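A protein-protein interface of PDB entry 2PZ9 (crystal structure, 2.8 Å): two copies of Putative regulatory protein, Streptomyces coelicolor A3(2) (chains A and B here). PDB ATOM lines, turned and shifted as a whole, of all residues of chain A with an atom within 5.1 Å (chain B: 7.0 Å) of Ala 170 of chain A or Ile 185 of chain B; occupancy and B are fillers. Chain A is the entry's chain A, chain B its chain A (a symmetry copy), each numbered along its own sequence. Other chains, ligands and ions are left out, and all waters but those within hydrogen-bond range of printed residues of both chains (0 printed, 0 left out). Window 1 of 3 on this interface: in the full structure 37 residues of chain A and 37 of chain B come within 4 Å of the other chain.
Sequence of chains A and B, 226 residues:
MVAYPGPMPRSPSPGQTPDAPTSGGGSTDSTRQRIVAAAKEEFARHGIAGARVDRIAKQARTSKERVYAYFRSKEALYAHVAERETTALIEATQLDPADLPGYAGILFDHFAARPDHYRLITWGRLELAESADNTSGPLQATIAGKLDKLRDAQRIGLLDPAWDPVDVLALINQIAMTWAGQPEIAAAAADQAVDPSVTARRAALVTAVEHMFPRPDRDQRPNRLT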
ATOM      1  N   GLN A 140     -32.900  -2.919 -17.164  1.00  0.00           N
ATOM      2  CA  GLN A 140     -32.745  -3.821 -16.016  1.00  0.00           C
ATOM      3  C   GLN A 140     -33.511  -5.140 -16.161  1.00  0.00           C
ATOM      4  O   GLN A 140     -33.007  -6.221 -15.811  1.00  0.00           O
ATOM      5  CB  GLN A 140     -33.193  -3.097 -14.737  1.00  0.00           C
ATOM      6  CG  GLN A 140     -32.262  -1.973 -14.294  1.00  0.00           C
ATOM      7  CD  GLN A 140     -30.844  -2.463 -13.984  1.00  0.00           C
ATOM      8  OE1 GLN A 140     -30.652  -3.464 -13.284  1.00  0.00           O
ATOM      9  NE2 GLN A 140     -29.849  -1.755 -14.505  1.00  0.00           N
ATOM     10  N   ILE A 143     -31.862  -7.405 -18.825  1.00  0.00           N
ATOM     11  CA  ILE A 143     -30.652  -7.872 -18.132  1.00  0.00           C
ATOM     12  C   ILE A 143     -30.956  -8.994 -17.126  1.00  0.00           C
ATOM     13  O   ILE A 143     -30.387 -10.079 -17.212  1.00  0.00           O
ATOM     14  CB  ILE A 143     -29.926  -6.711 -17.399  1.00  0.00           C
ATOM     15  CG1 ILE A 143     -29.315  -5.731 -18.397  1.00  0.00           C
ATOM     16  CG2 ILE A 143     -28.857  -7.233 -16.412  1.00  0.00           C
ATOM     17  CD1 ILE A 143     -29.203  -4.344 -17.843  1.00  0.00           C
ATOM     18  N   PRO A 165     -22.574 -15.446 -14.215  1.00  0.00           N
ATOM     19  CA  PRO A 165     -23.380 -14.867 -15.266  1.00  0.00           C
ATOM     20  C   PRO A 165     -23.127 -13.364 -15.381  1.00  0.00           C
ATOM     21  O   PRO A 165     -22.867 -12.859 -16.474  1.00  0.00           O
ATOM     22  CB  PRO A 165     -24.795 -15.132 -14.760  1.00  0.00           C
ATOM     23  CG  PRO A 165     -24.673 -16.431 -14.102  1.00  0.00           C
ATOM     24  CD  PRO A 165     -23.332 -16.448 -13.445  1.00  0.00           C
ATOM     25  N   VAL A 166     -23.206 -12.680 -14.239  1.00  0.00           N
ATOM     26  CA  VAL A 166     -22.951 -11.250 -14.128  1.00  0.00           C
ATOM     27  C   VAL A 166     -21.675 -10.856 -14.886  1.00  0.00           C
ATOM     28  O   VAL A 166     -21.685  -9.915 -15.679  1.00  0.00           O
ATOM     29  CB  VAL A 166     -22.918 -10.813 -12.623  1.00  0.00           C
ATOM     30  CG1 VAL A 166     -22.445  -9.395 -12.453  1.00  0.00           C
ATOM     31  CG2 VAL A 166     -24.298 -10.929 -12.022  1.00  0.00           C
ATOM     32  N   ASP A 167     -20.590 -11.585 -14.658  1.00  0.00           N
ATOM     33  CA  ASP A 167     -19.335 -11.292 -15.347  1.00  0.00           C
ATOM     34  C   ASP A 167     -19.425 -11.595 -16.860  1.00  0.00           C
ATOM     35  O   ASP A 167     -18.912 -10.823 -17.690  1.00  0.00           O
ATOM     36  CB  ASP A 167     -18.153 -12.030 -14.692  1.00  0.00           C
ATOM     37  CG  ASP A 167     -17.884 -11.564 -13.242  1.00  0.00           C
ATOM     38  OD1 ASP A 167     -17.645 -10.350 -13.027  1.00  0.00           O
ATOM     39  OD2 ASP A 167     -17.892 -12.414 -12.310  1.00  0.00           O
ATOM     40  N   VAL A 168     -20.082 -12.700 -17.213  1.00  0.00           N
ATOM     41  CA  VAL A 168     -20.190 -13.148 -18.601  1.00  0.00           C
ATOM     42  C   VAL A 168     -20.906 -12.090 -19.450  1.00  0.00           C
ATOM     43  O   VAL A 168     -20.412 -11.676 -20.510  1.00  0.00           O
ATOM     44  CB  VAL A 168     -20.925 -14.523 -18.694  1.00  0.00           C
ATOM     45  CG1 VAL A 168     -21.048 -14.978 -20.133  1.00  0.00           C
ATOM     46  CG2 VAL A 168     -20.219 -15.567 -17.861  1.00  0.00           C
ATOM     47  N   LEU A 169     -22.054 -11.645 -18.958  1.00  0.00           N
ATOM     48  CA  LEU A 169     -22.860 -10.651 -19.651  1.00  0.00           C
ATOM     49  C   LEU A 169     -22.104  -9.335 -19.863  1.00  0.00           C
ATOM     50  O   LEU A 169     -21.932  -8.885 -20.998  1.00  0.00           O
ATOM     51  CB  LEU A 169     -24.156 -10.410 -18.889  1.00  0.00           C
ATOM     52  CG  LEU A 169     -25.128  -9.452 -19.560  1.00  0.00           C
ATOM     53  CD1 LEU A 169     -25.737 -10.135 -20.765  1.00  0.00           C
ATOM     54  CD2 LEU A 169     -26.206  -8.925 -18.599  1.00  0.00           C
ATOM     55  N   ALA A 170     -21.636  -8.740 -18.761  1.00  0.00           N
ATOM     56  CA  ALA A 170     -20.858  -7.499 -18.777  1.00  0.00           C
ATOM     57  C   ALA A 170     -19.689  -7.532 -19.756  1.00  0.00           C
ATOM     58  O   ALA A 170     -19.580  -6.666 -20.631  1.00  0.00           O
ATOM     59  CB  ALA A 170     -20.362  -7.200 -17.394  1.00  0.00           C
ATOM     60  N   LEU A 171     -18.829  -8.531 -19.587  1.00  0.00           N
ATOM     61  CA  LEU A 171     -17.674  -8.734 -20.455  1.00  0.00           C
ATOM     62  C   LEU A 171     -18.027  -8.744 -21.940  1.00  0.00           C
ATOM     63  O   LEU A 171     -17.488  -7.958 -22.734  1.00  0.00           O
ATOM     64  CB  LEU A 171     -16.951 -10.042 -20.108  1.00  0.00           C
ATOM     65  CG  LEU A 171     -16.264 -10.049 -18.732  1.00  0.00           C
ATOM     66  CD1 LEU A 171     -15.999 -11.482 -18.256  1.00  0.00           C
ATOM     67  CD2 LEU A 171     -14.991  -9.162 -18.698  1.00  0.00           C
ATOM     68  N   ILE A 172     -18.942  -9.624 -22.315  1.00  0.00           N
ATOM     69  CA  ILE A 172     -19.270  -9.761 -23.716  1.00  0.00           C
ATOM     70  C   ILE A 172     -19.814  -8.439 -24.344  1.00  0.00           C
ATOM     71  O   ILE A 172     -19.396  -8.036 -25.440  1.00  0.00           O
ATOM     72  CB  ILE A 172     -20.182 -10.969 -23.932  1.00  0.00           C
ATOM     73  CG1 ILE A 172     -19.431 -12.236 -23.506  1.00  0.00           C
ATOM     74  CG2 ILE A 172     -20.603 -11.053 -25.406  1.00  0.00           C
ATOM     75  CD1 ILE A 172     -20.274 -13.480 -23.494  1.00  0.00           C
ATOM     76  N   ASN A 173     -20.726  -7.778 -23.643  1.00  0.00           N
ATOM     77  CA  ASN A 173     -21.092  -6.423 -23.969  1.00  0.00           C
ATOM     78  C   ASN A 173     -19.935  -5.428 -24.144  1.00  0.00           C
ATOM     79  O   ASN A 173     -19.952  -4.619 -25.078  1.00  0.00           O
ATOM     80  CB  ASN A 173     -22.020  -5.916 -22.906  1.00  0.00           C
ATOM     81  CG  ASN A 173     -23.408  -6.340 -23.148  1.00  0.00           C
ATOM     82  OD1 ASN A 173     -24.184  -5.574 -23.718  1.00  0.00           O
ATOM     83  ND2 ASN A 173     -23.741  -7.577 -22.784  1.00  0.00           N
ATOM     84  N   GLN A 174     -18.957  -5.474 -23.241  1.00  0.00           N
ATOM     85  CA  GLN A 174     -17.783  -4.604 -23.340  1.00  0.00           C
ATOM     86  C   GLN A 174     -17.036  -4.847 -24.620  1.00  0.00           C
ATOM     87  O   GLN A 174     -16.967  -3.957 -25.448  1.00  0.00           O
ATOM     88  CB  GLN A 174     -16.811  -4.817 -22.193  1.00  0.00           C
ATOM     89  CG  GLN A 174     -16.916  -3.796 -21.163  1.00  0.00           C
ATOM     90  CD  GLN A 174     -16.625  -2.382 -21.636  1.00  0.00           C
ATOM     91  OE1 GLN A 174     -15.511  -2.058 -22.024  1.00  0.00           O
ATOM     92  NE2 GLN A 174     -17.623  -1.519 -21.541  1.00  0.00           N
ATOM     93  N   THR B 178     -14.326  -2.707 -18.455  1.00  0.00           N
ATOM     94  CA  THR B 178     -15.600  -3.403 -18.428  1.00  0.00           C
ATOM     95  C   THR B 178     -16.636  -2.863 -17.430  1.00  0.00           C
ATOM     96  O   THR B 178     -17.807  -2.746 -17.770  1.00  0.00           O
ATOM     97  CB  THR B 178     -15.333  -4.898 -18.206  1.00  0.00           C
ATOM     98  OG1 THR B 178     -16.467  -5.659 -18.573  1.00  0.00           O
ATOM     99  CG2 THR B 178     -15.013  -5.160 -16.774  1.00  0.00           C
ATOM    100  N   TRP B 179     -16.196  -2.516 -16.224  1.00  0.00           N
ATOM    101  CA  TRP B 179     -17.103  -2.110 -15.139  1.00  0.00           C
ATOM    102  C   TRP B 179     -17.343  -0.608 -15.072  1.00  0.00           C
ATOM    103  O   TRP B 179     -18.417  -0.151 -14.654  1.00  0.00           O
ATOM    104  CB  TRP B 179     -16.635  -2.678 -13.801  1.00  0.00           C
ATOM    105  CG  TRP B 179     -16.811  -4.149 -13.827  1.00  0.00           C
ATOM    106  CD1 TRP B 179     -15.832  -5.101 -13.963  1.00  0.00           C
ATOM    107  CD2 TRP B 179     -18.062  -4.860 -13.806  1.00  0.00           C
ATOM    108  NE1 TRP B 179     -16.396  -6.370 -13.999  1.00  0.00           N
ATOM    109  CE2 TRP B 179     -17.761  -6.246 -13.907  1.00  0.00           C
ATOM    110  CE3 TRP B 179     -19.407  -4.462 -13.695  1.00  0.00           C
ATOM    111  CZ2 TRP B 179     -18.750  -7.220 -13.899  1.00  0.00           C
ATOM    112  CZ3 TRP B 179     -20.375  -5.423 -13.686  1.00  0.00           C
ATOM    113  CH2 TRP B 179     -20.049  -6.788 -13.787  1.00  0.00           C
ATOM    114  N   GLN B 182     -19.723  -0.501 -18.345  1.00  0.00           N
ATOM    115  CA  GLN B 182     -21.071  -1.123 -18.238  1.00  0.00           C
ATOM    116  C   GLN B 182     -21.742  -0.797 -16.891  1.00  0.00           C
ATOM    117  O   GLN B 182     -21.906  -1.698 -16.063  1.00  0.00           O
ATOM    118  CB  GLN B 182     -20.989  -2.660 -18.370  1.00  0.00           C
ATOM    119  CG  GLN B 182     -20.298  -3.206 -19.623  1.00  0.00           C
ATOM    120  CD  GLN B 182     -21.117  -3.013 -20.899  1.00  0.00           C
ATOM    121  OE1 GLN B 182     -20.548  -2.912 -21.978  1.00  0.00           O
ATOM    122  NE2 GLN B 182     -22.449  -2.965 -20.780  1.00  0.00           N
ATOM    123  N   PRO B 183     -22.127   0.480 -16.658  1.00  0.00           N
ATOM    124  CA  PRO B 183     -22.658   0.855 -15.330  1.00  0.00           C
ATOM    125  C   PRO B 183     -24.030   0.260 -15.051  1.00  0.00           C
ATOM    126  O   PRO B 183     -24.350  -0.038 -13.889  1.00  0.00           O
ATOM    127  CB  PRO B 183     -22.759   2.385 -15.396  1.00  0.00           C
ATOM    128  CG  PRO B 183     -22.867   2.692 -16.837  1.00  0.00           C
ATOM    129  CD  PRO B 183     -22.107   1.629 -17.583  1.00  0.00           C
ATOM    130  N   GLU B 184     -24.830   0.098 -16.107  1.00  0.00           N
ATOM    131  CA  GLU B 184     -26.169  -0.474 -15.972  1.00  0.00           C
ATOM    132  C   GLU B 184     -26.100  -1.912 -15.408  1.00  0.00           C
ATOM    133  O   GLU B 184     -26.663  -2.166 -14.357  1.00  0.00           O
ATOM    134  CB  GLU B 184     -26.952  -0.402 -17.296  1.00  0.00           C
ATOM    135  CG  GLU B 184     -26.496  -1.355 -18.430  1.00  0.00           C
ATOM    136  CD  GLU B 184     -25.027  -1.209 -18.815  1.00  0.00           C
ATOM    137  OE1 GLU B 184     -24.337  -2.248 -18.917  1.00  0.00           O
ATOM    138  OE2 GLU B 184     -24.565  -0.062 -19.009  1.00  0.00           O
ATOM    139  N   ILE B 185     -25.361  -2.817 -16.062  1.00  0.00           N
ATOM    140  CA  ILE B 185     -25.065  -4.151 -15.516  1.00  0.00           C
ATOM    141  C   ILE B 185     -24.336  -4.028 -14.172  1.00  0.00           C
ATOM    142  O   ILE B 185     -24.649  -4.765 -13.230  1.00  0.00           O
ATOM    143  CB  ILE B 185     -24.217  -5.033 -16.500  1.00  0.00           C
ATOM    144  CG1 ILE B 185     -24.903  -5.171 -17.866  1.00  0.00           C
ATOM    145  CG2 ILE B 185     -23.939  -6.430 -15.924  1.00  0.00           C
ATOM    146  CD1 ILE B 185     -23.949  -5.564 -19.029  1.00  0.00           C
ATOM    147  N   ALA B 186     -23.373  -3.103 -14.074  1.00  0.00           N
ATOM    148  CA  ALA B 186     -22.685  -2.864 -12.800  1.00  0.00           C
ATOM    149  C   ALA B 186     -23.707  -2.621 -11.695  1.00  0.00           C
ATOM    150  O   ALA B 186     -23.551  -3.131 -10.591  1.00  0.00           O
ATOM    151  CB  ALA B 186     -21.689  -1.710 -12.896  1.00  0.00           C
ATOM    152  N   ALA B 187     -24.769  -1.871 -11.995  1.00  0.00           N
ATOM    153  CA  ALA B 187     -25.850  -1.667 -11.012  1.00  0.00           C
ATOM    154  C   ALA B 187     -26.503  -3.001 -10.590  1.00  0.00           C
ATOM    155  O   ALA B 187     -26.607  -3.296  -9.388  1.00  0.00           O
ATOM    156  CB  ALA B 187     -26.892  -0.660 -11.521  1.00  0.00           C
ATOM    157  N   ALA B 188     -26.906  -3.806 -11.585  1.00  0.00           N
ATOM    158  CA  ALA B 188     -27.537  -5.118 -11.354  1.00  0.00           C
ATOM    159  C   ALA B 188     -26.599  -6.045 -10.609  1.00  0.00           C
ATOM    160  O   ALA B 188     -27.034  -6.873  -9.818  1.00  0.00           O
ATOM    161  CB  ALA B 188     -27.975  -5.757 -12.675  1.00  0.00           C
ATOM    162  N   ALA B 189     -25.304  -5.877 -10.865  1.00  0.00           N
ATOM    163  CA  ALA B 189     -24.253  -6.676 -10.250  1.00  0.00           C
ATOM    164  C   ALA B 189     -24.382  -6.633  -8.743  1.00  0.00           C
ATOM    165  O   ALA B 189     -23.958  -7.566  -8.070  1.00  0.00           O
ATOM    166  CB  ALA B 189     -22.881  -6.166 -10.688  1.00  0.00           C
ATOM    167  N   ALA B 190     -24.999  -5.551  -8.253  1.00  0.00           N
ATOM    168  CA  ALA B 190     -25.205  -5.259  -6.826  1.00  0.00           C
ATOM    169  C   ALA B 190     -25.369  -6.516  -5.994  1.00  0.00           C
ATOM    170  O   ALA B 190     -24.438  -6.949  -5.319  1.00  0.00           O
ATOM    171  CB  ALA B 190     -26.409  -4.334  -6.635  1.00  0.00           C
ATOM    172  N   GLN B 192     -26.944  -9.266  -7.546  1.00  0.00           N
ATOM    173  CA  GLN B 192     -27.087 -10.333  -8.530  1.00  0.00           C
ATOM    174  C   GLN B 192     -25.791 -11.167  -8.654  1.00  0.00           C
ATOM    175  O   GLN B 192     -25.765 -12.179  -9.363  1.00  0.00           O
ATOM    176  CB  GLN B 192     -27.493  -9.764  -9.898  1.00  0.00           C
ATOM    177  CG  GLN B 192     -29.008  -9.682 -10.134  1.00  0.00           C
ATOM    178  CD  GLN B 192     -29.585 -10.843 -10.978  1.00  0.00           C
ATOM    179  OE1 GLN B 192     -29.199 -12.005 -10.844  1.00  0.00           O
ATOM    180  NE2 GLN B 192     -30.532 -10.514 -11.841  1.00  0.00           N
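OE1 of Gln 182 of chain B sits at hydrogen-bond distance from NE2 of Gln 174 of chain A (3.3 Å).
NE2 of Gln 140 of chain A sits at hydrogen-bond distance from O of Glu 184 of chain B, at 3.2 Å.
ND2 of Asn 173 of chain A lies within hydrogen-bond range of O of Leu 169 of chain A.
NE2 of Gln 182 of chain B is in hydrogen-bond range of OE1 of Glu 184 of chain B (2.7 Å).
CB of Ala 188 of chain B touches OE1 of Gln 140 of chain A, at 3.6 Å.
Trp 179 of chain B touches Val 166 of chain A (CH2 to CG1, 3.8 Å).
Val 166 of chain A touches Ala 189 of chain B (CG1 to CB, 3.7 Å).
CG2 of Val 166 of chain A touches O of Gln 192 of chain B, 3.3 Å away.
CZ2 of Trp 179 of chain B touches OD1 of Asp 167 of chain A, at 3.4 Å.
Trp 179 of chain B touches Ala 170 of chain A.
Gln 182 of chain B touches Ala 170 of chain A.
CA of Ala 170 of chain A touches CD1 of Ile 185 of chain B, at 3.7 Å.
CA of Leu 171 of chain A touches OG1 of Thr 178 of chain B, 3.8 Å away.
OE1 of Gln 182 of chain B touches C of Asn 173 of chain A (3.4 Å).
Of chain B, only Thr 178, Trp 179, Gln 182 and Ile 185 come within 4 Å of Ala 170 of chain A.
Of chain A, only Ala 170 comes within 4 Å of Ile 185 of chain B.
Of the printed residues of chain A, Gln 182 of chain B touches Ala 170, Asn 173 and Gln 174.
Of the printed residues of chain B, Val 166 of chain A touches Trp 179, Ala 189 and Gln 192.
Of the printed residues of chain A, Thr 178 of chain B touches Ala 170, Leu 171 and Gln 174.
Pro 183 of chain B touches none of the printed residues of chain A.
Ala 190 of chain B touches none of the printed residues of chain A.
The nearest residue of chain B that does not touch Ala 170 of chain A is Ala 186 of chain B (6.1 Å).
The nearest printed residue of chain A that does not touch Ala 189 of chain B is Gln 140 of chain A (6.3 Å).
Of the 12 printed residues of chain B, 8 touch a printed residue of chain A.
Printed residues of chain B that touch a printed residue of chain A: Thr 178, Trp 179, Gln 182, Glu 184, Ile 185, Ala 188, Ala 189 and Gln 192.
Among the printed residues, 14 pairs touch across the chains.
Among the printed residues, no Asp or Glu carboxylate lies within 4 Å of a Lys or Arg side-chain nitrogen of the other chain.
No position is printed for both chains.
Of the 14 pairs that touch across the chains among the printed residues, none has its exchanged pair printed and touching as well.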
